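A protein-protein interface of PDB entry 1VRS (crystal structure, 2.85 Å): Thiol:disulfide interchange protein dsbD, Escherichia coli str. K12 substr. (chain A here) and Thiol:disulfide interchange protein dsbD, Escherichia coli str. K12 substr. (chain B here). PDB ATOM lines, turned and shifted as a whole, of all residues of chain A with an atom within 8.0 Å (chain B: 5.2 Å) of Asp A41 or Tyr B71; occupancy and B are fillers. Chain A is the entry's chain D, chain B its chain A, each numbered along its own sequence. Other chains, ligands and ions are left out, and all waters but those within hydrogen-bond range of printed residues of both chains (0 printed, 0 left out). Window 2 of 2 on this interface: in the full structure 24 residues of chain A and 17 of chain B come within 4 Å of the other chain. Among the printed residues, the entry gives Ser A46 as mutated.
OH of Tyr B71 sits at hydrogen-bond distance from O of Asp A41.
The side-chain carboxylate (OD1) of Asp B68 is in hydrogen-bond range of the backbone NH (N) of Phe B70 (2.5 Å).
The side-chain carboxylate (OD1) of Asp B68 lies within hydrogen-bond range of the backbone NH (N) of Tyr B71.
OD1 of Asp A41 is in hydrogen-bond range of OH of Tyr A39.
The backbone NH (N) of Asp A41 is in hydrogen-bond range of the side-chain hydroxyl (OG1) of Thr A74 (2.8 Å).
The indole nitrogen (NE1) of Trp A42 lies within hydrogen-bond range of the backbone carbonyl oxygen (O) of Thr A74.
Trp A42 touches Tyr B71 (CA to OH, 3.8 Å).
OD2 of Asp B68 touches CG2 of Val A44, 3.5 Å away.
Tyr B71 touches Val A44.
Lys A47 touches Phe B70 (CD to CD2, 3.3 Å).
Tyr B71 touches Lys A47 (OH to NZ, 3.5 Å).
Of chain B, only Tyr B71 (3.1 Å) comes within 4 Å of Asp A41.
Of the printed residues of chain B, Val A44 touches Asp B68 (3.5 Å) and Tyr B71 (3.9 Å).
Of the printed residues of chain B, Lys A47 touches Phe B70 and Tyr B71.
Of the printed residues of chain A, Asp B68 touches Val A44.
Of the printed residues of chain A, Phe B70 touches Lys A47.
Tyr B71 touches four residues of chain A.
Gly B72 touches none of the printed residues of chain A.
The nearest printed residue of chain B that does not touch Asp A41 is Phe B70 (6.8 Å).
The nearest residue of chain A that does not touch Tyr B71 is Cys A43 (5.4 Å).
The nearest printed residue of chain B that does not touch Val A44 is Phe B70 (4.1 Å).
Of the 14 printed residues of chain A, 4 touch a printed residue of chain B.
Printed residues of chain A that touch a printed residue of chain B: Asp A41, Trp A42, Val A44 and Lys A47.
Of the 7 printed residues of chain B, 3 touch a printed residue of chain A.
Hydrophobic or aromatic side chains of chain B that line the printed part of chain A: Phe B70 and Tyr B71.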
ATOM      1  N   TYR A  39       0.192  11.672  27.128  1.00  0.00           N
ATOM      2  CA  TYR A  39       1.200  12.133  26.186  1.00  0.00           C
ATOM      3  C   TYR A  39       1.639  11.095  25.151  1.00  0.00           C
ATOM      4  O   TYR A  39       1.502   9.897  25.375  1.00  0.00           O
ATOM      5  CB  TYR A  39       2.397  12.573  27.038  1.00  0.00           C
ATOM      6  CG  TYR A  39       3.697  12.789  26.311  1.00  0.00           C
ATOM      7  CD1 TYR A  39       4.558  11.725  26.024  1.00  0.00           C
ATOM      8  CD2 TYR A  39       4.059  14.065  25.886  1.00  0.00           C
ATOM      9  CE1 TYR A  39       5.745  11.933  25.325  1.00  0.00           C
ATOM     10  CE2 TYR A  39       5.239  14.288  25.190  1.00  0.00           C
ATOM     11  CZ  TYR A  39       6.076  13.227  24.906  1.00  0.00           C
ATOM     12  OH  TYR A  39       7.220  13.486  24.178  1.00  0.00           O
ATOM     13  N   ALA A  40       2.174  11.564  24.026  1.00  0.00           N
ATOM     14  CA  ALA A  40       2.693  10.680  22.978  1.00  0.00           C
ATOM     15  C   ALA A  40       3.785  11.407  22.187  1.00  0.00           C
ATOM     16  O   ALA A  40       3.600  12.555  21.798  1.00  0.00           O
ATOM     17  CB  ALA A  40       1.569  10.239  22.048  1.00  0.00           C
ATOM     18  N   ASP A  41       4.917  10.744  21.951  1.00  0.00           N
ATOM     19  CA  ASP A  41       6.027  11.358  21.214  1.00  0.00           C
ATOM     20  C   ASP A  41       5.666  11.837  19.803  1.00  0.00           C
ATOM     21  O   ASP A  41       6.077  12.921  19.377  1.00  0.00           O
ATOM     22  CB  ASP A  41       7.205  10.388  21.108  1.00  0.00           C
ATOM     23  CG  ASP A  41       7.760   9.979  22.462  1.00  0.00           C
ATOM     24  OD1 ASP A  41       7.984  10.868  23.308  1.00  0.00           O
ATOM     25  OD2 ASP A  41       7.989   8.767  22.676  1.00  0.00           O
ATOM     26  N   TRP A  42       4.903  11.034  19.068  1.00  0.00           N
ATOM     27  CA  TRP A  42       4.534  11.422  17.719  1.00  0.00           C
ATOM     28  C   TRP A  42       3.600  12.611  17.668  1.00  0.00           C
ATOM     29  O   TRP A  42       3.514  13.277  16.650  1.00  0.00           O
ATOM     30  CB  TRP A  42       3.916  10.247  16.966  1.00  0.00           C
ATOM     31  CG  TRP A  42       3.086   9.316  17.800  1.00  0.00           C
ATOM     32  CD1 TRP A  42       3.503   8.173  18.415  1.00  0.00           C
ATOM     33  CD2 TRP A  42       1.688   9.441  18.090  1.00  0.00           C
ATOM     34  NE1 TRP A  42       2.451   7.573  19.068  1.00  0.00           N
ATOM     35  CE2 TRP A  42       1.327   8.333  18.885  1.00  0.00           C
ATOM     36  CE3 TRP A  42       0.708  10.385  17.758  1.00  0.00           C
ATOM     37  CZ2 TRP A  42       0.026   8.142  19.353  1.00  0.00           C
ATOM     38  CZ3 TRP A  42      -0.583  10.195  18.226  1.00  0.00           C
ATOM     39  CH2 TRP A  42      -0.914   9.082  19.015  1.00  0.00           C
ATOM     40  N   CYS A  43       2.910  12.890  18.768  1.00  0.00           N
ATOM     41  CA  CYS A  43       1.984  14.019  18.820  1.00  0.00           C
ATOM     42  C   CYS A  43       2.662  15.374  19.046  1.00  0.00           C
ATOM     43  O   CYS A  43       3.157  15.656  20.135  1.00  0.00           O
ATOM     44  CB  CYS A  43       0.965  13.788  19.922  1.00  0.00           C
ATOM     45  SG  CYS A  43      -0.383  15.002  19.940  1.00  0.00           S
ATOM     46  N   VAL A  44       2.663  16.215  18.019  1.00  0.00           N
ATOM     47  CA  VAL A  44       3.280  17.531  18.107  1.00  0.00           C
ATOM     48  C   VAL A  44       2.669  18.401  19.192  1.00  0.00           C
ATOM     49  O   VAL A  44       3.377  19.067  19.949  1.00  0.00           O
ATOM     50  CB  VAL A  44       3.177  18.253  16.761  1.00  0.00           C
ATOM     51  CG1 VAL A  44       3.451  19.746  16.925  1.00  0.00           C
ATOM     52  CG2 VAL A  44       4.167  17.631  15.807  1.00  0.00           C
ATOM     53  N   ALA A  45       1.344  18.395  19.252  1.00  0.00           N
ATOM     54  CA  ALA A  45       0.620  19.174  20.249  1.00  0.00           C
ATOM     55  C   ALA A  45       1.037  18.730  21.653  1.00  0.00           C
ATOM     56  O   ALA A  45       1.134  19.535  22.579  1.00  0.00           O
ATOM     57  CB  ALA A  45      -0.879  18.987  20.063  1.00  0.00           C
ATOM     58  N   SER A  46       1.278  17.434  21.798  1.00  0.00           N
ATOM     59  CA  SER A  46       1.688  16.869  23.068  1.00  0.00           C
ATOM     60  C   SER A  46       3.082  17.401  23.401  1.00  0.00           C
ATOM     61  O   SER A  46       3.409  17.636  24.560  1.00  0.00           O
ATOM     62  CB  SER A  46       1.701  15.343  22.965  1.00  0.00           C
ATOM     63  OG  SER A  46       1.124  14.751  24.111  1.00  0.00           O
ATOM     64  N   LYS A  47       3.904  17.588  22.375  1.00  0.00           N
ATOM     65  CA  LYS A  47       5.251  18.112  22.566  1.00  0.00           C
ATOM     66  C   LYS A  47       5.174  19.591  22.897  1.00  0.00           C
ATOM     67  O   LYS A  47       5.914  20.078  23.739  1.00  0.00           O
ATOM     68  CB  LYS A  47       6.095  17.935  21.303  1.00  0.00           C
ATOM     69  CG  LYS A  47       6.871  16.644  21.241  1.00  0.00           C
ATOM     70  CD  LYS A  47       7.454  16.448  19.859  1.00  0.00           C
ATOM     71  CE  LYS A  47       8.448  15.308  19.829  1.00  0.00           C
ATOM     72  NZ  LYS A  47       7.865  14.041  20.348  1.00  0.00           N
ATOM     73  N   ASN A  72       2.458   7.693  29.224  1.00  0.00           N
ATOM     74  CA  ASN A  72       3.065   7.875  27.906  1.00  0.00           C
ATOM     75  C   ASN A  72       2.542   6.767  27.018  1.00  0.00           C
ATOM     76  O   ASN A  72       2.979   5.624  27.124  1.00  0.00           O
ATOM     77  CB  ASN A  72       4.587   7.793  27.961  1.00  0.00           C
ATOM     78  CG  ASN A  72       5.217   8.118  26.627  1.00  0.00           C
ATOM     79  OD1 ASN A  72       4.787   7.608  25.596  1.00  0.00           O
ATOM     80  ND2 ASN A  72       6.237   8.973  26.635  1.00  0.00           N
ATOM     81  N   VAL A  73       1.607   7.114  26.143  1.00  0.00           N
ATOM     82  CA  VAL A  73       0.988   6.143  25.253  1.00  0.00           C
ATOM     83  C   VAL A  73       1.590   6.095  23.853  1.00  0.00           C
ATOM     84  O   VAL A  73       0.932   5.676  22.903  1.00  0.00           O
ATOM     85  CB  VAL A  73      -0.530   6.418  25.124  1.00  0.00           C
ATOM     86  CG1 VAL A  73      -1.209   6.211  26.464  1.00  0.00           C
ATOM     87  CG2 VAL A  73      -0.769   7.835  24.617  1.00  0.00           C
ATOM     88  N   THR A  74       2.847   6.502  23.731  1.00  0.00           N
ATOM     89  CA  THR A  74       3.519   6.532  22.442  1.00  0.00           C
ATOM     90  C   THR A  74       3.480   5.210  21.692  1.00  0.00           C
ATOM     91  O   THR A  74       3.272   5.189  20.480  1.00  0.00           O
ATOM     92  CB  THR A  74       4.983   6.966  22.591  1.00  0.00           C
ATOM     93  OG1 THR A  74       5.036   8.270  23.179  1.00  0.00           O
ATOM     94  CG2 THR A  74       5.658   7.015  21.239  1.00  0.00           C
ATOM     95  N   ALA A  75       3.673   4.106  22.405  1.00  0.00           N
ATOM     96  CA  ALA A  75       3.669   2.789  21.762  1.00  0.00           C
ATOM     97  C   ALA A  75       2.282   2.360  21.289  1.00  0.00           C
ATOM     98  O   ALA A  75       2.147   1.486  20.436  1.00  0.00           O
ATOM     99  CB  ALA A  75       4.239   1.746  22.711  1.00  0.00           C
ATOM    100  N   LEU A  92      -4.720  13.051  21.738  1.00  0.00           N
ATOM    101  CA  LEU A  92      -3.776  13.772  22.579  1.00  0.00           C
ATOM    102  C   LEU A  92      -3.439  15.105  21.953  1.00  0.00           C
ATOM    103  O   LEU A  92      -3.564  15.265  20.741  1.00  0.00           O
ATOM    104  CB  LEU A  92      -2.516  12.938  22.740  1.00  0.00           C
ATOM    105  CG  LEU A  92      -2.818  11.444  22.924  1.00  0.00           C
ATOM    106  CD1 LEU A  92      -1.605  10.648  22.550  1.00  0.00           C
ATOM    107  CD2 LEU A  92      -3.238  11.141  24.345  1.00  0.00           C
ATOM    108  N   ASP B  68       5.943  22.019  11.181  1.00  0.00           N
ATOM    109  CA  ASP B  68       5.951  22.252  12.608  1.00  0.00           C
ATOM    110  C   ASP B  68       7.411  22.226  13.018  1.00  0.00           C
ATOM    111  O   ASP B  68       8.235  21.579  12.375  1.00  0.00           O
ATOM    112  CB  ASP B  68       5.167  21.172  13.348  1.00  0.00           C
ATOM    113  CG  ASP B  68       5.840  19.825  13.291  1.00  0.00           C
ATOM    114  OD1 ASP B  68       6.953  19.669  13.844  1.00  0.00           O
ATOM    115  OD2 ASP B  68       5.244  18.917  12.683  1.00  0.00           O
ATOM    116  N   GLU B  69       7.725  22.931  14.092  1.00  0.00           N
ATOM    117  CA  GLU B  69       9.083  23.028  14.587  1.00  0.00           C
ATOM    118  C   GLU B  69       9.753  21.716  14.972  1.00  0.00           C
ATOM    119  O   GLU B  69      10.940  21.706  15.254  1.00  0.00           O
ATOM    120  CB  GLU B  69       9.104  23.952  15.791  1.00  0.00           C
ATOM    121  CG  GLU B  69       8.133  23.520  16.873  1.00  0.00           C
ATOM    122  CD  GLU B  69       8.509  24.061  18.226  1.00  0.00           C
ATOM    123  OE1 GLU B  69       8.637  25.292  18.354  1.00  0.00           O
ATOM    124  OE2 GLU B  69       8.681  23.258  19.161  1.00  0.00           O
ATOM    125  N   PHE B  70       9.021  20.608  14.990  1.00  0.00           N
ATOM    126  CA  PHE B  70       9.641  19.350  15.396  1.00  0.00           C
ATOM    127  C   PHE B  70      10.079  18.424  14.277  1.00  0.00           C
ATOM    128  O   PHE B  70      11.243  18.030  14.204  1.00  0.00           O
ATOM    129  CB  PHE B  70       8.719  18.570  16.341  1.00  0.00           C
ATOM    130  CG  PHE B  70       8.486  19.246  17.664  1.00  0.00           C
ATOM    131  CD1 PHE B  70       7.471  20.193  17.812  1.00  0.00           C
ATOM    132  CD2 PHE B  70       9.284  18.933  18.770  1.00  0.00           C
ATOM    133  CE1 PHE B  70       7.246  20.815  19.036  1.00  0.00           C
ATOM    134  CE2 PHE B  70       9.070  19.551  20.005  1.00  0.00           C
ATOM    135  CZ  PHE B  70       8.045  20.495  20.140  1.00  0.00           C
ATOM    136  N   TYR B  71       9.147  18.067  13.407  1.00  0.00           N
ATOM    137  CA  TYR B  71       9.456  17.156  12.318  1.00  0.00           C
ATOM    138  C   TYR B  71       9.631  17.887  11.007  1.00  0.00           C
ATOM    139  O   TYR B  71       9.797  17.266   9.965  1.00  0.00           O
ATOM    140  CB  TYR B  71       8.342  16.124  12.215  1.00  0.00           C
ATOM    141  CG  TYR B  71       8.214  15.302  13.469  1.00  0.00           C
ATOM    142  CD1 TYR B  71       9.105  14.266  13.731  1.00  0.00           C
ATOM    143  CD2 TYR B  71       7.221  15.571  14.408  1.00  0.00           C
ATOM    144  CE1 TYR B  71       9.016  13.513  14.896  1.00  0.00           C
ATOM    145  CE2 TYR B  71       7.120  14.822  15.581  1.00  0.00           C
ATOM    146  CZ  TYR B  71       8.023  13.792  15.817  1.00  0.00           C
ATOM    147  OH  TYR B  71       7.945  13.035  16.963  1.00  0.00           O
ATOM    148  N   GLY B  72       9.597  19.214  11.073  1.00  0.00           N
ATOM    149  CA  GLY B  72       9.758  20.019   9.882  1.00  0.00           C
ATOM    150  C   GLY B  72       8.556  19.927   8.974  1.00  0.00           C
ATOM    151  O   GLY B  72       7.517  20.533   9.245  1.00  0.00           O
ATOM    152  N   LYS B  73       8.691  19.155   7.901  1.00  0.00           N
ATOM    153  CA  LYS B  73       7.610  18.988   6.937  1.00  0.00           C
ATOM    154  C   LYS B  73       7.029  17.584   6.855  1.00  0.00           C
ATOM    155  O   LYS B  73       7.709  16.585   7.112  1.00  0.00           O
ATOM    156  CB  LYS B  73       8.069  19.405   5.539  1.00  0.00           C
ATOM    157  CG  LYS B  73       8.032  20.895   5.289  1.00  0.00           C
ATOM    158  CD  LYS B  73       8.076  21.201   3.797  1.00  0.00           C
ATOM    159  CE  LYS B  73       8.054  22.711   3.561  1.00  0.00           C
ATOM    160  NZ  LYS B  73       7.000  23.394   4.375  1.00  0.00           N
ATOM    161  N   SER B  74       5.763  17.532   6.466  1.00  0.00           N
ATOM    162  CA  SER B  74       5.049  16.287   6.332  1.00  0.00           C
ATOM    163  C   SER B  74       3.980  16.460   5.277  1.00  0.00           C
ATOM    164  O   SER B  74       3.322  17.506   5.215  1.00  0.00           O
ATOM    165  CB  SER B  74       4.408  15.922   7.665  1.00  0.00           C
ATOM    166  OG  SER B  74       5.396  15.587   8.621  1.00  0.00           O
